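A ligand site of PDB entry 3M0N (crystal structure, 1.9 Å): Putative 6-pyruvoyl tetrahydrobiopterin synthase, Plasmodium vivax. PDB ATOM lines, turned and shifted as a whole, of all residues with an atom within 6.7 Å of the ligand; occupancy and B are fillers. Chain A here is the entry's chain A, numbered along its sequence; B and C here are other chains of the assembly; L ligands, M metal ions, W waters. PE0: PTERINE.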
ATOM      1  N   HIS A  36      -5.600 -21.950  30.023  1.00  0.00           N
ATOM      2  CA  HIS A  36      -4.811 -20.710  29.842  1.00  0.00           C
ATOM      3  C   HIS A  36      -5.724 -19.523  30.122  1.00  0.00           C
ATOM      4  O   HIS A  36      -6.911 -19.703  30.406  1.00  0.00           O
ATOM      5  CB  HIS A  36      -4.217 -20.643  28.455  1.00  0.00           C
ATOM      6  CG  HIS A  36      -5.105 -20.014  27.413  1.00  0.00           C
ATOM      7  ND1 HIS A  36      -4.679 -18.971  26.621  1.00  0.00           N
ATOM      8  CD2 HIS A  36      -6.365 -20.300  27.028  1.00  0.00           C
ATOM      9  CE1 HIS A  36      -5.657 -18.632  25.796  1.00  0.00           C
ATOM     10  NE2 HIS A  36      -6.691 -19.423  26.022  1.00  0.00           N
ATOM     11  N   ILE A  38      -5.845 -15.273  28.555  1.00  0.00           N
ATOM     12  CA  ILE A  38      -5.223 -14.167  27.817  1.00  0.00           C
ATOM     13  C   ILE A  38      -5.118 -12.951  28.723  1.00  0.00           C
ATOM     14  O   ILE A  38      -6.077 -12.619  29.414  1.00  0.00           O
ATOM     15  CB  ILE A  38      -6.087 -13.767  26.588  1.00  0.00           C
ATOM     16  CG1 ILE A  38      -6.225 -14.948  25.623  1.00  0.00           C
ATOM     17  CG2 ILE A  38      -5.474 -12.557  25.854  1.00  0.00           C
ATOM     18  CD1 ILE A  38      -4.889 -15.452  25.092  1.00  0.00           C
ATOM     19  N   HIS A  48      -9.809 -20.500  31.420  1.00  0.00           N
ATOM     20  CA  HIS A  48     -10.562 -21.428  30.591  1.00  0.00           C
ATOM     21  C   HIS A  48      -9.569 -22.372  29.949  1.00  0.00           C
ATOM     22  O   HIS A  48      -8.453 -22.500  30.442  1.00  0.00           O
ATOM     23  CB  HIS A  48     -11.411 -20.662  29.560  1.00  0.00           C
ATOM     24  CG  HIS A  48     -10.617 -19.868  28.560  1.00  0.00           C
ATOM     25  ND1 HIS A  48     -10.152 -18.595  28.816  1.00  0.00           N
ATOM     26  CD2 HIS A  48     -10.261 -20.160  27.290  1.00  0.00           C
ATOM     27  CE1 HIS A  48      -9.522 -18.146  27.749  1.00  0.00           C
ATOM     28  NE2 HIS A  48      -9.584 -19.068  26.805  1.00  0.00           N
ATOM     29  N   HIS A  50      -8.727 -25.163  26.154  1.00  0.00           N
ATOM     30  CA  HIS A  50      -8.925 -25.571  24.758  1.00  0.00           C
ATOM     31  C   HIS A  50      -8.298 -26.924  24.465  1.00  0.00           C
ATOM     32  O   HIS A  50      -7.326 -27.319  25.117  1.00  0.00           O
ATOM     33  CB  HIS A  50      -8.267 -24.582  23.787  1.00  0.00           C
ATOM     34  CG  HIS A  50      -8.729 -23.175  23.933  1.00  0.00           C
ATOM     35  ND1 HIS A  50      -9.979 -22.748  23.540  1.00  0.00           N
ATOM     36  CD2 HIS A  50      -8.076 -22.076  24.384  1.00  0.00           C
ATOM     37  CE1 HIS A  50     -10.094 -21.459  23.775  1.00  0.00           C
ATOM     38  NE2 HIS A  50      -8.956 -21.020  24.273  1.00  0.00           N
ATOM     39  N   TYR A  52      -6.186 -27.750  21.879  1.00  0.00           N
ATOM     40  CA  TYR A  52      -5.377 -27.173  20.809  1.00  0.00           C
ATOM     41  C   TYR A  52      -5.029 -28.280  19.855  1.00  0.00           C
ATOM     42  O   TYR A  52      -4.807 -29.413  20.271  1.00  0.00           O
ATOM     43  CB  TYR A  52      -4.090 -26.574  21.366  1.00  0.00           C
ATOM     44  CG  TYR A  52      -4.249 -25.323  22.191  1.00  0.00           C
ATOM     45  CD1 TYR A  52      -4.103 -24.062  21.617  1.00  0.00           C
ATOM     46  CD2 TYR A  52      -4.491 -25.397  23.564  1.00  0.00           C
ATOM     47  CE1 TYR A  52      -4.201 -22.920  22.376  1.00  0.00           C
ATOM     48  CE2 TYR A  52      -4.605 -24.244  24.336  1.00  0.00           C
ATOM     49  CZ  TYR A  52      -4.464 -23.006  23.726  1.00  0.00           C
ATOM     50  OH  TYR A  52      -4.565 -21.849  24.477  1.00  0.00           O
ATOM     51  N   SER A 132      -0.131 -16.293  25.943  1.00  0.00           N
ATOM     52  CA  SER A 132      -0.581 -17.612  25.537  1.00  0.00           C
ATOM     53  C   SER A 132      -1.577 -17.508  24.358  1.00  0.00           C
ATOM     54  O   SER A 132      -2.659 -18.132  24.377  1.00  0.00           O
ATOM     55  CB  SER A 132      -1.179 -18.394  26.732  1.00  0.00           C
ATOM     56  OG  SER A 132      -2.218 -17.672  27.384  1.00  0.00           O
ATOM     57  N   SER A 133      -1.231 -16.718  23.340  1.00  0.00           N
ATOM     58  CA  SER A 133      -1.986 -16.651  22.112  1.00  0.00           C
ATOM     59  C   SER A 133      -1.600 -17.774  21.153  1.00  0.00           C
ATOM     60  O   SER A 133      -0.492 -18.322  21.205  1.00  0.00           O
ATOM     61  CB  SER A 133      -1.769 -15.302  21.398  1.00  0.00           C
ATOM     62  OG  SER A 133      -0.437 -15.188  20.945  1.00  0.00           O
ATOM     63  N   THR A 134      -2.505 -18.060  20.239  1.00  0.00           N
ATOM     64  CA  THR A 134      -2.293 -19.056  19.207  1.00  0.00           C
ATOM     65  C   THR A 134      -1.065 -18.764  18.354  1.00  0.00           C
ATOM     66  O   THR A 134      -0.303 -19.655  18.026  1.00  0.00           O
ATOM     67  CB  THR A 134      -3.550 -19.103  18.330  1.00  0.00           C
ATOM     68  OG1 THR A 134      -4.682 -19.329  19.171  1.00  0.00           O
ATOM     69  CG2 THR A 134      -3.434 -20.194  17.319  1.00  0.00           C
ATOM     70  N   GLU A 135      -0.882 -17.494  18.012  1.00  0.00           N
ATOM     71  CA  GLU A 135       0.280 -17.062  17.232  1.00  0.00           C
ATOM     72  C   GLU A 135       1.628 -17.381  17.923  1.00  0.00           C
ATOM     73  O   GLU A 135       2.573 -17.896  17.297  1.00  0.00           O
ATOM     74  CB  GLU A 135       0.222 -15.557  17.008  1.00  0.00           C
ATOM     75  CG  GLU A 135      -0.845 -15.077  16.039  1.00  0.00           C
ATOM     76  CD  GLU A 135      -2.148 -14.668  16.709  1.00  0.00           C
ATOM     77  OE1 GLU A 135      -2.542 -15.320  17.690  1.00  0.00           O
ATOM     78  OE2 GLU A 135      -2.781 -13.706  16.233  1.00  0.00           O
ATOM     79  N   GLU A 168      -6.826 -23.064  18.173  1.00  0.00           N
ATOM     80  CA  GLU A 168      -7.420 -22.989  19.514  1.00  0.00           C
ATOM     81  C   GLU A 168      -8.729 -23.774  19.577  1.00  0.00           C
ATOM     82  O   GLU A 168      -9.071 -24.370  20.600  1.00  0.00           O
ATOM     83  CB  GLU A 168      -7.727 -21.539  19.874  1.00  0.00           C
ATOM     84  CG  GLU A 168      -6.901 -20.945  21.010  1.00  0.00           C
ATOM     85  CD  GLU A 168      -7.381 -19.540  21.377  1.00  0.00           C
ATOM     86  OE1 GLU A 168      -8.265 -19.028  20.651  1.00  0.00           O
ATOM     87  OE2 GLU A 168      -6.878 -18.965  22.381  1.00  0.00           O
ATOM     88  N   GLN A 172     -10.637 -21.218  14.522  1.00  0.00           N
ATOM     89  CA  GLN A 172      -9.602 -20.162  14.592  1.00  0.00           C
ATOM     90  C   GLN A 172      -8.209 -20.753  14.685  1.00  0.00           C
ATOM     91  O   GLN A 172      -7.903 -21.499  15.620  1.00  0.00           O
ATOM     92  CB  GLN A 172      -9.859 -19.152  15.730  1.00  0.00           C
ATOM     93  CG  GLN A 172     -10.651 -19.671  16.928  1.00  0.00           C
ATOM     94  CD  GLN A 172     -11.045 -18.561  17.903  1.00  0.00           C
ATOM     95  OE1 GLN A 172     -11.828 -17.664  17.561  1.00  0.00           O
ATOM     96  NE2 GLN A 172     -10.508 -18.627  19.124  1.00  0.00           N
ATOM     97  N   ALA A 174      -3.760 -20.127  13.685  1.00  0.00           N
ATOM     98  CA  ALA A 174      -2.605 -19.294  13.318  1.00  0.00           C
ATOM     99  C   ALA A 174      -1.536 -20.181  12.690  1.00  0.00           C
ATOM    100  O   ALA A 174      -1.285 -21.288  13.162  1.00  0.00           O
ATOM    101  CB  ALA A 174      -2.024 -18.567  14.552  1.00  0.00           C
ATOM    102  N   LEU B  23      -3.485 -15.844   9.790  1.00  0.00           N
ATOM    103  CA  LEU B  23      -4.664 -16.215  10.551  1.00  0.00           C
ATOM    104  C   LEU B  23      -5.736 -16.743   9.606  1.00  0.00           C
ATOM    105  O   LEU B  23      -5.886 -16.246   8.488  1.00  0.00           O
ATOM    106  CB  LEU B  23      -5.214 -15.030  11.348  1.00  0.00           C
ATOM    107  CG  LEU B  23      -4.403 -14.447  12.493  1.00  0.00           C
ATOM    108  CD1 LEU B  23      -5.264 -13.459  13.292  1.00  0.00           C
ATOM    109  CD2 LEU B  23      -3.824 -15.531  13.411  1.00  0.00           C
ATOM    110  N   GLY B  66      -0.023  -9.626  21.426  1.00  0.00           N
ATOM    111  CA  GLY B  66       0.077 -11.074  21.148  1.00  0.00           C
ATOM    112  C   GLY B  66      -0.796 -11.614  20.027  1.00  0.00           C
ATOM    113  O   GLY B  66      -0.758 -12.818  19.732  1.00  0.00           O
ATOM    114  N   TYR B  67      -1.583 -10.742  19.416  1.00  0.00           N
ATOM    115  CA  TYR B  67      -2.432 -11.072  18.262  1.00  0.00           C
ATOM    116  C   TYR B  67      -1.941 -10.358  16.988  1.00  0.00           C
ATOM    117  O   TYR B  67      -1.411  -9.256  17.084  1.00  0.00           O
ATOM    118  CB  TYR B  67      -3.839 -10.572  18.512  1.00  0.00           C
ATOM    119  CG  TYR B  67      -4.597 -11.127  19.695  1.00  0.00           C
ATOM    120  CD1 TYR B  67      -4.251 -12.343  20.297  1.00  0.00           C
ATOM    121  CD2 TYR B  67      -5.714 -10.446  20.189  1.00  0.00           C
ATOM    122  CE1 TYR B  67      -4.997 -12.840  21.368  1.00  0.00           C
ATOM    123  CE2 TYR B  67      -6.446 -10.931  21.251  1.00  0.00           C
ATOM    124  CZ  TYR B  67      -6.091 -12.135  21.836  1.00  0.00           C
ATOM    125  OH  TYR B  67      -6.835 -12.619  22.881  1.00  0.00           O
ATOM    126  N   VAL B  68      -2.118 -10.948  15.804  1.00  0.00           N
ATOM    127  CA  VAL B  68      -2.038 -10.164  14.554  1.00  0.00           C
ATOM    128  C   VAL B  68      -3.269  -9.236  14.516  1.00  0.00           C
ATOM    129  O   VAL B  68      -3.140  -8.030  14.279  1.00  0.00           O
ATOM    130  CB  VAL B  68      -2.009 -11.019  13.248  1.00  0.00           C
ATOM    131  CG1 VAL B  68      -1.912 -10.092  12.025  1.00  0.00           C
ATOM    132  CG2 VAL B  68      -0.862 -12.011  13.252  1.00  0.00           C
ATOM    133  N   ILE B  69      -4.433  -9.827  14.743  1.00  0.00           N
ATOM    134  CA  ILE B  69      -5.707  -9.110  14.959  1.00  0.00           C
ATOM    135  C   ILE B  69      -6.623 -10.069  15.734  1.00  0.00           C
ATOM    136  O   ILE B  69      -6.529 -11.286  15.582  1.00  0.00           O
ATOM    137  CB  ILE B  69      -6.323  -8.650  13.612  1.00  0.00           C
ATOM    138  CG1 ILE B  69      -7.646  -7.910  13.827  1.00  0.00           C
ATOM    139  CG2 ILE B  69      -6.518  -9.820  12.663  1.00  0.00           C
ATOM    140  CD1 ILE B  69      -8.117  -7.172  12.566  1.00  0.00           C
ATOM    141  N   ASP B  70      -7.491  -9.518  16.579  1.00  0.00           N
ATOM    142  CA  ASP B  70      -8.379 -10.371  17.419  1.00  0.00           C
ATOM    143  C   ASP B  70      -9.373 -11.207  16.572  1.00  0.00           C
ATOM    144  O   ASP B  70     -10.184 -10.654  15.811  1.00  0.00           O
ATOM    145  CB  ASP B  70      -9.132  -9.482  18.426  1.00  0.00           C
ATOM    146  CG  ASP B  70      -9.873 -10.276  19.512  1.00  0.00           C
ATOM    147  OD1 ASP B  70     -10.160 -11.481  19.333  1.00  0.00           O
ATOM    148  OD2 ASP B  70     -10.171  -9.673  20.564  1.00  0.00           O
ATOM    149  N   PHE B  71      -9.309 -12.543  16.723  1.00  0.00           N
ATOM    150  CA  PHE B  71     -10.237 -13.458  16.042  1.00  0.00           C
ATOM    151  C   PHE B  71     -11.704 -12.995  16.147  1.00  0.00           C
ATOM    152  O   PHE B  71     -12.462 -13.083  15.174  1.00  0.00           O
ATOM    153  CB  PHE B  71     -10.162 -14.879  16.630  1.00  0.00           C
ATOM    154  CG  PHE B  71      -8.954 -15.691  16.206  1.00  0.00           C
ATOM    155  CD1 PHE B  71      -8.613 -15.824  14.865  1.00  0.00           C
ATOM    156  CD2 PHE B  71      -8.198 -16.362  17.164  1.00  0.00           C
ATOM    157  CE1 PHE B  71      -7.513 -16.591  14.485  1.00  0.00           C
ATOM    158  CE2 PHE B  71      -7.088 -17.138  16.789  1.00  0.00           C
ATOM    159  CZ  PHE B  71      -6.748 -17.249  15.451  1.00  0.00           C
ATOM    160  N   SER B  72     -12.093 -12.521  17.323  1.00  0.00           N
ATOM    161  CA  SER B  72     -13.489 -12.109  17.593  1.00  0.00           C
ATOM    162  C   SER B  72     -14.016 -11.061  16.598  1.00  0.00           C
ATOM    163  O   SER B  72     -15.195 -11.097  16.206  1.00  0.00           O
ATOM    164  CB  SER B  72     -13.614 -11.549  19.009  1.00  0.00           C
ATOM    165  OG  SER B  72     -12.864 -10.354  19.120  1.00  0.00           O
ATOM    166  N   LEU B  74     -12.784 -10.604  13.459  1.00  0.00           N
ATOM    167  CA  LEU B  74     -12.889 -11.279  12.167  1.00  0.00           C
ATOM    168  C   LEU B  74     -14.174 -12.090  12.076  1.00  0.00           C
ATOM    169  O   LEU B  74     -14.884 -12.030  11.073  1.00  0.00           O
ATOM    170  CB  LEU B  74     -11.687 -12.206  11.907  1.00  0.00           C
ATOM    171  CG  LEU B  74     -10.288 -11.588  11.935  1.00  0.00           C
ATOM    172  CD1 LEU B  74      -9.238 -12.679  11.678  1.00  0.00           C
ATOM    173  CD2 LEU B  74     -10.155 -10.450  10.928  1.00  0.00           C
ATOM    174  N   HIS C  87     -15.748 -20.151  28.920  1.00  0.00           N
ATOM    175  CA  HIS C  87     -14.687 -19.304  29.476  1.00  0.00           C
ATOM    176  C   HIS C  87     -14.613 -19.270  31.019  1.00  0.00           C
ATOM    177  O   HIS C  87     -14.342 -18.224  31.609  1.00  0.00           O
ATOM    178  CB  HIS C  87     -14.731 -17.906  28.840  1.00  0.00           C
ATOM    179  CG  HIS C  87     -13.991 -17.814  27.537  1.00  0.00           C
ATOM    180  ND1 HIS C  87     -13.080 -16.820  27.259  1.00  0.00           N
ATOM    181  CD2 HIS C  87     -13.993 -18.646  26.463  1.00  0.00           C
ATOM    182  CE1 HIS C  87     -12.575 -17.016  26.054  1.00  0.00           C
ATOM    183  NE2 HIS C  87     -13.110 -18.112  25.546  1.00  0.00           N
HETATM  184  C1  PE0 L   1      -6.955 -15.345  20.462  1.00  0.00           C
HETATM  185  C4  PE0 L   1      -5.713 -15.708  19.914  1.00  0.00           C
HETATM  186  O4  PE0 L   1      -4.997 -16.584  20.427  1.00  0.00           O
HETATM  187  N2  PE0 L   1      -5.269 -15.044  18.777  1.00  0.00           N
HETATM  188  C3  PE0 L   1      -6.059 -14.040  18.194  1.00  0.00           C
HETATM  189  N6  PE0 L   1      -5.629 -13.415  17.100  1.00  0.00           N
HETATM  190  N1  PE0 L   1      -7.261 -13.715  18.736  1.00  0.00           N
HETATM  191  C2  PE0 L   1      -7.704 -14.344  19.851  1.00  0.00           C
HETATM  192  N3  PE0 L   1      -8.897 -14.007  20.375  1.00  0.00           N
HETATM  193  C6  PE0 L   1      -9.355 -14.620  21.465  1.00  0.00           C
HETATM  194  C5  PE0 L   1      -8.598 -15.615  22.072  1.00  0.00           C
HETATM  195  N4  PE0 L   1      -7.425 -15.962  21.573  1.00  0.00           N
HETATM  196 ZN    ZN M   1      -8.593 -19.255  25.091  1.00  0.00          ZN
HETATM  197  O   HOH W   1      -9.965 -17.621  23.595  1.00  0.00           O
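The backbone carbonyl oxygen of Ile 69 of chain B is in hydrogen-bond range of a nitrogen (N6) of the ligand (2.8 Å). O4 of the ligand lies within hydrogen-bond range of N of Thr 134 (2.9 Å). OG1 of Thr 134 is in hydrogen-bond range of O4 of the ligand (3.0 Å). A nitrogen (N2) of the ligand lies within hydrogen-bond range of the side-chain carboxylate (OE1) of Glu 135. The backbone NH (N) of Phe 71 of chain B is in hydrogen-bond range of a nitrogen (N1) of the ligand (3.1 Å). The side-chain carboxylate (OE2) of Glu 168 lies close to a nitrogen (N4) of the ligand (3.2 Å).
N of Val 68 of chain B sits at hydrogen-bond distance from OE2 of Glu 135 (2.9 Å). OG of Ser 72 of chain B lies within hydrogen-bond range of OD1 of Asp 70 of chain B (2.9 Å). The side-chain carboxylate of Glu 168 lies within hydrogen-bond range of the side-chain amide nitrogen of Gln 172, at 2.7 Å. A ring nitrogen (ND1) of His 50 lies close to the backbone carbonyl oxygen (O) of Glu 168 (3.5 Å). The side-chain hydroxyl (OG) of Ser 133 sits at hydrogen-bond distance from the backbone carbonyl oxygen (O) of Gly 66 of chain B, at 2.7 Å.
OD1 of Asp 70 of chain B lies close to N3 of the ligand. Ser 133 touches the ligand. Leu 23 of chain B touches the ligand. CD1 of Tyr 67 of chain B touches C3 of the ligand, at 3.3 Å. Hydrophobic or aromatic side chains that line the ligand: Leu 23 of chain B, Tyr 67 of chain B and Phe 71 of chain B. Of the 22 residues printed, 9 come within 4 Å of the ligand. The nearest printed residue that does not touch the ligand is Ile 38 (4.3 Å).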
